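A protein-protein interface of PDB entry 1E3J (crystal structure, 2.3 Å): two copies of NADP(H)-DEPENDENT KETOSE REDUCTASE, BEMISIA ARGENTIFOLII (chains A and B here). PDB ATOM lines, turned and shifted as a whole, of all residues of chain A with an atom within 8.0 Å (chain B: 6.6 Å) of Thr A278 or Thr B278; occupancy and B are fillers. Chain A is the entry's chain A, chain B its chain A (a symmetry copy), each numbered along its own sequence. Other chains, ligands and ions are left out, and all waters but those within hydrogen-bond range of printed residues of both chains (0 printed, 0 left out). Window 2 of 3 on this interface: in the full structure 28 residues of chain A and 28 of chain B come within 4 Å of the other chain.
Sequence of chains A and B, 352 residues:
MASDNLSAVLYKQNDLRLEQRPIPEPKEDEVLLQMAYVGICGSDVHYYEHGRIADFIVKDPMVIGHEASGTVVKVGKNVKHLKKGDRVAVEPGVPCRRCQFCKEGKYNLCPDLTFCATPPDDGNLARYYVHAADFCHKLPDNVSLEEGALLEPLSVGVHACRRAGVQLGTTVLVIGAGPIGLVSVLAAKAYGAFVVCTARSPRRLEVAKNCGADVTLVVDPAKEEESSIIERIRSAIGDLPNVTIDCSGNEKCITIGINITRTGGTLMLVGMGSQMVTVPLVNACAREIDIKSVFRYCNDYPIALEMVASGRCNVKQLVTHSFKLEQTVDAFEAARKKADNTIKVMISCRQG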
ATOM      1  N   ASN A 250      15.882 -20.061   8.906  1.00  0.00           N
ATOM      2  CA  ASN A 250      15.878 -21.513   8.832  1.00  0.00           C
ATOM      3  C   ASN A 250      17.179 -22.074   8.239  1.00  0.00           C
ATOM      4  O   ASN A 250      17.624 -21.655   7.158  1.00  0.00           O
ATOM      5  CB  ASN A 250      14.702 -21.982   7.984  1.00  0.00           C
ATOM      6  CG  ASN A 250      14.659 -23.485   7.879  1.00  0.00           C
ATOM      7  OD1 ASN A 250      14.087 -24.164   8.739  1.00  0.00           O
ATOM      8  ND2 ASN A 250      15.308 -24.025   6.848  1.00  0.00           N
ATOM      9  N   GLU A 251      17.765 -23.062   8.910  1.00  0.00           N
ATOM     10  CA  GLU A 251      19.019 -23.630   8.437  1.00  0.00           C
ATOM     11  C   GLU A 251      18.990 -24.272   7.039  1.00  0.00           C
ATOM     12  O   GLU A 251      20.020 -24.297   6.338  1.00  0.00           O
ATOM     13  CB  GLU A 251      19.570 -24.634   9.453  1.00  0.00           C
ATOM     14  CG  GLU A 251      18.843 -25.954   9.480  1.00  0.00           C
ATOM     15  CD  GLU A 251      19.078 -26.718  10.774  1.00  0.00           C
ATOM     16  OE1 GLU A 251      20.252 -27.002  11.122  1.00  0.00           O
ATOM     17  OE2 GLU A 251      18.071 -27.029  11.445  1.00  0.00           O
ATOM     18  N   LYS A 252      17.848 -24.808   6.623  1.00  0.00           N
ATOM     19  CA  LYS A 252      17.816 -25.421   5.287  1.00  0.00           C
ATOM     20  C   LYS A 252      17.862 -24.310   4.242  1.00  0.00           C
ATOM     21  O   LYS A 252      18.530 -24.439   3.212  1.00  0.00           O
ATOM     22  CB  LYS A 252      16.581 -26.315   5.088  1.00  0.00           C
ATOM     23  CG  LYS A 252      16.628 -27.623   5.898  1.00  0.00           C
ATOM     24  CD  LYS A 252      15.628 -28.654   5.349  1.00  0.00           C
ATOM     25  CE  LYS A 252      15.495 -29.884   6.260  1.00  0.00           C
ATOM     26  NZ  LYS A 252      14.593 -29.611   7.447  1.00  0.00           N
ATOM     27  N   CYS A 253      17.179 -23.207   4.542  1.00  0.00           N
ATOM     28  CA  CYS A 253      17.179 -22.045   3.671  1.00  0.00           C
ATOM     29  C   CYS A 253      18.564 -21.396   3.655  1.00  0.00           C
ATOM     30  O   CYS A 253      19.015 -20.922   2.617  1.00  0.00           O
ATOM     31  CB  CYS A 253      16.128 -21.044   4.136  1.00  0.00           C
ATOM     32  SG  CYS A 253      14.453 -21.625   3.795  1.00  0.00           S
ATOM     33  N   ILE A 254      19.258 -21.397   4.788  1.00  0.00           N
ATOM     34  CA  ILE A 254      20.590 -20.787   4.812  1.00  0.00           C
ATOM     35  C   ILE A 254      21.574 -21.665   4.049  1.00  0.00           C
ATOM     36  O   ILE A 254      22.504 -21.166   3.380  1.00  0.00           O
ATOM     37  CB  ILE A 254      21.093 -20.594   6.242  1.00  0.00           C
ATOM     38  CG1 ILE A 254      20.296 -19.463   6.895  1.00  0.00           C
ATOM     39  CG2 ILE A 254      22.590 -20.309   6.240  1.00  0.00           C
ATOM     40  CD1 ILE A 254      20.463 -19.363   8.398  1.00  0.00           C
ATOM     41  N   THR A 255      21.341 -22.971   4.120  1.00  0.00           N
ATOM     42  CA  THR A 255      22.223 -23.911   3.454  1.00  0.00           C
ATOM     43  C   THR A 255      22.017 -23.695   1.971  1.00  0.00           C
ATOM     44  O   THR A 255      22.956 -23.690   1.211  1.00  0.00           O
ATOM     45  CB  THR A 255      21.885 -25.392   3.832  1.00  0.00           C
ATOM     46  OG1 THR A 255      22.042 -25.581   5.250  1.00  0.00           O
ATOM     47  CG2 THR A 255      22.814 -26.364   3.094  1.00  0.00           C
ATOM     48  N   ILE A 258      23.743 -20.444   0.865  1.00  0.00           N
ATOM     49  CA  ILE A 258      25.162 -20.676   0.703  1.00  0.00           C
ATOM     50  C   ILE A 258      25.488 -21.446  -0.585  1.00  0.00           C
ATOM     51  O   ILE A 258      26.502 -21.180  -1.266  1.00  0.00           O
ATOM     52  CB  ILE A 258      25.682 -21.513   1.871  1.00  0.00           C
ATOM     53  CG1 ILE A 258      25.566 -20.706   3.162  1.00  0.00           C
ATOM     54  CG2 ILE A 258      27.139 -21.969   1.604  1.00  0.00           C
ATOM     55  CD1 ILE A 258      25.951 -21.473   4.397  1.00  0.00           C
ATOM     56  N   SER A 274      16.838 -19.758  14.893  1.00  0.00           N
ATOM     57  CA  SER A 274      16.363 -20.369  16.128  1.00  0.00           C
ATOM     58  C   SER A 274      17.400 -20.065  17.202  1.00  0.00           C
ATOM     59  O   SER A 274      17.213 -19.175  18.036  1.00  0.00           O
ATOM     60  CB  SER A 274      16.205 -21.894  15.955  1.00  0.00           C
ATOM     61  OG  SER A 274      17.399 -22.502  15.472  1.00  0.00           O
ATOM     62  N   GLN A 275      18.503 -20.796  17.174  1.00  0.00           N
ATOM     63  CA  GLN A 275      19.558 -20.580  18.151  1.00  0.00           C
ATOM     64  C   GLN A 275      20.843 -20.974  17.455  1.00  0.00           C
ATOM     65  O   GLN A 275      21.779 -20.188  17.363  1.00  0.00           O
ATOM     66  N   MET A 276      20.851 -22.208  16.962  1.00  0.00           N
ATOM     67  CA  MET A 276      21.977 -22.788  16.245  1.00  0.00           C
ATOM     68  C   MET A 276      21.445 -23.306  14.914  1.00  0.00           C
ATOM     69  O   MET A 276      20.264 -23.650  14.786  1.00  0.00           O
ATOM     70  CB  MET A 276      22.564 -23.984  17.014  1.00  0.00           C
ATOM     71  CG  MET A 276      23.212 -23.662  18.355  1.00  0.00           C
ATOM     72  SD  MET A 276      24.820 -22.854  18.197  1.00  0.00           S
ATOM     73  CE  MET A 276      25.964 -24.221  18.439  1.00  0.00           C
ATOM     74  N   VAL A 277      22.318 -23.351  13.922  1.00  0.00           N
ATOM     75  CA  VAL A 277      21.943 -23.886  12.640  1.00  0.00           C
ATOM     76  C   VAL A 277      23.106 -24.743  12.201  1.00  0.00           C
ATOM     77  O   VAL A 277      24.265 -24.461  12.535  1.00  0.00           O
ATOM     78  CB  VAL A 277      21.666 -22.784  11.598  1.00  0.00           C
ATOM     79  CG1 VAL A 277      20.412 -22.043  11.975  1.00  0.00           C
ATOM     80  CG2 VAL A 277      22.848 -21.820  11.507  1.00  0.00           C
ATOM     81  N   THR A 278      22.800 -25.819  11.494  1.00  0.00           N
ATOM     82  CA  THR A 278      23.836 -26.704  10.988  1.00  0.00           C
ATOM     83  C   THR A 278      23.956 -26.283   9.539  1.00  0.00           C
ATOM     84  O   THR A 278      23.042 -26.485   8.764  1.00  0.00           O
ATOM     85  CB  THR A 278      23.402 -28.169  11.095  1.00  0.00           C
ATOM     86  OG1 THR A 278      23.369 -28.551  12.480  1.00  0.00           O
ATOM     87  CG2 THR A 278      24.361 -29.062  10.341  1.00  0.00           C
ATOM     88  N   VAL A 279      25.084 -25.681   9.180  1.00  0.00           N
ATOM     89  CA  VAL A 279      25.246 -25.178   7.820  1.00  0.00           C
ATOM     90  C   VAL A 279      26.565 -25.545   7.219  1.00  0.00           C
ATOM     91  O   VAL A 279      27.516 -25.849   7.925  1.00  0.00           O
ATOM     92  CB  VAL A 279      25.097 -23.642   7.784  1.00  0.00           C
ATOM     93  CG1 VAL A 279      23.683 -23.244   8.221  1.00  0.00           C
ATOM     94  CG2 VAL A 279      26.142 -23.012   8.687  1.00  0.00           C
ATOM     95  N   PRO A 280      26.647 -25.503   5.886  1.00  0.00           N
ATOM     96  CA  PRO A 280      27.871 -25.845   5.172  1.00  0.00           C
ATOM     97  C   PRO A 280      28.842 -24.692   4.974  1.00  0.00           C
ATOM     98  O   PRO A 280      29.163 -24.361   3.823  1.00  0.00           O
ATOM     99  CB  PRO A 280      27.339 -26.358   3.846  1.00  0.00           C
ATOM    100  CG  PRO A 280      26.243 -25.372   3.588  1.00  0.00           C
ATOM    101  CD  PRO A 280      25.531 -25.338   4.936  1.00  0.00           C
ATOM    102  N   LEU A 281      29.322 -24.092   6.066  1.00  0.00           N
ATOM    103  CA  LEU A 281      30.271 -22.994   5.953  1.00  0.00           C
ATOM    104  C   LEU A 281      31.455 -23.354   5.069  1.00  0.00           C
ATOM    105  O   LEU A 281      31.983 -22.483   4.371  1.00  0.00           O
ATOM    106  CB  LEU A 281      30.797 -22.556   7.321  1.00  0.00           C
ATOM    107  CG  LEU A 281      29.844 -21.906   8.318  1.00  0.00           C
ATOM    108  CD1 LEU A 281      30.705 -21.221   9.395  1.00  0.00           C
ATOM    109  CD2 LEU A 281      28.921 -20.903   7.630  1.00  0.00           C
ATOM    110  N   GLU B 251      33.785 -26.595  14.398  1.00  0.00           N
ATOM    111  CA  GLU B 251      32.594 -25.859  14.796  1.00  0.00           C
ATOM    112  C   GLU B 251      32.607 -25.258  16.212  1.00  0.00           C
ATOM    113  O   GLU B 251      31.953 -24.228  16.463  1.00  0.00           O
ATOM    114  CB  GLU B 251      31.344 -26.725  14.616  1.00  0.00           C
ATOM    115  CG  GLU B 251      31.175 -27.799  15.661  1.00  0.00           C
ATOM    116  CD  GLU B 251      30.241 -28.908  15.206  1.00  0.00           C
ATOM    117  OE1 GLU B 251      29.065 -28.625  14.858  1.00  0.00           O
ATOM    118  OE2 GLU B 251      30.696 -30.072  15.195  1.00  0.00           O
ATOM    119  N   LYS B 252      33.316 -25.882  17.147  1.00  0.00           N
ATOM    120  CA  LYS B 252      33.333 -25.309  18.501  1.00  0.00           C
ATOM    121  C   LYS B 252      34.178 -24.037  18.480  1.00  0.00           C
ATOM    122  O   LYS B 252      33.834 -23.041  19.121  1.00  0.00           O
ATOM    123  CB  LYS B 252      33.862 -26.305  19.546  1.00  0.00           C
ATOM    124  CG  LYS B 252      32.892 -27.464  19.840  1.00  0.00           C
ATOM    125  CD  LYS B 252      33.245 -28.162  21.163  1.00  0.00           C
ATOM    126  CE  LYS B 252      32.436 -29.451  21.380  1.00  0.00           C
ATOM    127  NZ  LYS B 252      33.006 -30.612  20.590  1.00  0.00           N
ATOM    128  N   THR B 255      32.202 -21.356  16.802  1.00  0.00           N
ATOM    129  CA  THR B 255      31.146 -20.881  17.677  1.00  0.00           C
ATOM    130  C   THR B 255      31.800 -19.899  18.624  1.00  0.00           C
ATOM    131  O   THR B 255      31.249 -18.865  18.918  1.00  0.00           O
ATOM    132  CB  THR B 255      30.493 -22.052  18.485  1.00  0.00           C
ATOM    133  OG1 THR B 255      29.909 -23.005  17.579  1.00  0.00           O
ATOM    134  CG2 THR B 255      29.400 -21.519  19.420  1.00  0.00           C
ATOM    135  N   MET B 276      29.808 -29.831   7.412  1.00  0.00           N
ATOM    136  CA  MET B 276      28.773 -29.010   8.020  1.00  0.00           C
ATOM    137  C   MET B 276      29.237 -28.673   9.433  1.00  0.00           C
ATOM    138  O   MET B 276      30.012 -29.415  10.048  1.00  0.00           O
ATOM    139  CB  MET B 276      27.449 -29.784   8.134  1.00  0.00           C
ATOM    140  CG  MET B 276      26.781 -30.161   6.817  1.00  0.00           C
ATOM    141  SD  MET B 276      25.998 -28.760   5.987  1.00  0.00           S
ATOM    142  CE  MET B 276      24.269 -28.956   6.444  1.00  0.00           C
ATOM    143  N   VAL B 277      28.769 -27.545   9.940  1.00  0.00           N
ATOM    144  CA  VAL B 277      29.087 -27.161  11.290  1.00  0.00           C
ATOM    145  C   VAL B 277      27.798 -26.641  11.880  1.00  0.00           C
ATOM    146  O   VAL B 277      26.955 -26.079  11.168  1.00  0.00           O
ATOM    147  CB  VAL B 277      30.182 -26.078  11.354  1.00  0.00           C
ATOM    148  CG1 VAL B 277      31.493 -26.664  10.908  1.00  0.00           C
ATOM    149  CG2 VAL B 277      29.807 -24.882  10.478  1.00  0.00           C
ATOM    150  N   THR B 278      27.616 -26.870  13.170  1.00  0.00           N
ATOM    151  CA  THR B 278      26.430 -26.389  13.858  1.00  0.00           C
ATOM    152  C   THR B 278      26.931 -25.147  14.562  1.00  0.00           C
ATOM    153  O   THR B 278      27.735 -25.239  15.469  1.00  0.00           O
ATOM    154  CB  THR B 278      25.929 -27.424  14.870  1.00  0.00           C
ATOM    155  OG1 THR B 278      25.396 -28.556  14.162  1.00  0.00           O
ATOM    156  CG2 THR B 278      24.860 -26.825  15.755  1.00  0.00           C
ATOM    157  N   VAL B 279      26.464 -23.981  14.130  1.00  0.00           N
ATOM    158  CA  VAL B 279      26.956 -22.735  14.707  1.00  0.00           C
ATOM    159  C   VAL B 279      25.858 -21.778  15.044  1.00  0.00           C
ATOM    160  O   VAL B 279      24.759 -21.869  14.515  1.00  0.00           O
ATOM    161  CB  VAL B 279      27.941 -22.038  13.744  1.00  0.00           C
ATOM    162  CG1 VAL B 279      29.172 -22.923  13.525  1.00  0.00           C
ATOM    163  CG2 VAL B 279      27.239 -21.747  12.429  1.00  0.00           C
ATOM    164  N   PRO B 280      26.149 -20.821  15.930  1.00  0.00           N
ATOM    165  CA  PRO B 280      25.168 -19.829  16.354  1.00  0.00           C
ATOM    166  C   PRO B 280      25.092 -18.588  15.480  1.00  0.00           C
ATOM    167  O   PRO B 280      25.311 -17.477  15.985  1.00  0.00           O
ATOM    168  CB  PRO B 280      25.634 -19.494  17.759  1.00  0.00           C
ATOM    169  CG  PRO B 280      27.116 -19.447  17.555  1.00  0.00           C
ATOM    170  CD  PRO B 280      27.361 -20.729  16.765  1.00  0.00           C
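The backbone nitrogen (N) of Pro B280 lies close to the side-chain sulfur (SD) of Met A276 (3.3 Å).
OG1 of Thr B278 is in hydrogen-bond range of OG1 of Thr A278 (2.6 Å).
N of Val A279 lies within hydrogen-bond range of O of Val B277 (2.8 Å).
O of Val B277 sits close to O of Val A277 (3.4 Å).
SD of Met B276 lies close to N of Pro A280, 3.3 Å away.
The backbone NH (N) of Val B279 is in hydrogen-bond range of the backbone carbonyl oxygen (O) of Val A277.
N of Thr B278 is in hydrogen-bond range of OE1 of Glu B251 (2.8 Å).
The backbone NH (N) of Thr A278 sits at hydrogen-bond distance from the side-chain carboxylate (OE1) of Glu A251.
O of Met A276 is in hydrogen-bond range of OG of Ser A274, 3.2 Å away.
Among the printed residues, merely in contact across the chains: Thr A278 with Val B277 (3.2 Å), Val A277 with Thr B278 (3.2 Å), Met A276 with Val B279 (3.4 Å), Val A279 with Met B276 (3.4 Å), Gln A275 with Pro B280 (3.6 Å), Met A276 with Thr B278 (3.6 Å), Thr A278 with Met B276 (3.6 Å) and Leu A281 with Val B277 (3.7 Å).
Ile A254 touches none of the printed residues of chain B.
Of the printed residues of chain B, Gln A275 touches Pro B280.
Printed residues of chain B within 4 Å of Met A276: Thr B278 (3.6 Å), Val B279 (3.4 Å) and Pro B280 (3.3 Å).
Thr A278 touches just these residues of chain B: Met B276 (3.6 Å), Val B277 (3.2 Å) and Thr B278 (2.6 Å).
Of the printed residues of chain B, Val A279 touches Met B276 and Val B277.
Thr B255 touches none of the printed residues of chain A.
Thr B278 touches three residues of chain A.
Printed residues of chain A within 4 Å of Pro B280: Gln A275 and Met A276.
The nearest residue of chain A that does not touch Thr B278 is Val A279 (4.9 Å).
Of the 8 printed residues of chain B, 5 touch a printed residue of chain A.
Hydrophobic or aromatic side chains of chain B that line the printed part of chain A: Met B276, Val B277 and Pro B280.
Of the 15 printed residues of chain A, 7 touch a printed residue of chain B.
Printed residues of chain A that touch a printed residue of chain B: Gln A275, Met A276, Val A277, Thr A278, Val A279, Pro A280 and Leu A281.
Hydrophobic or aromatic side chains of chain A within 4 Å of the printed part of chain B: Met A276, Val A277, Pro A280 and Leu A281.
Among the printed residues, 14 pairs touch across the chains.
Among the printed residues, no Asp or Glu carboxylate lies within 4 Å of a Lys or Arg side-chain nitrogen of the other chain.
Met A276 touches Thr B278, and with the chains exchanged Thr A278 touches Met B276.
Val A277 touches Thr B278, and with the chains exchanged Thr A278 touches Val B277.
Val A277 touches Val B279, and with the chains exchanged Val A279 touches Val B277.
Thr A278 touches its own counterpart, Thr B278.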
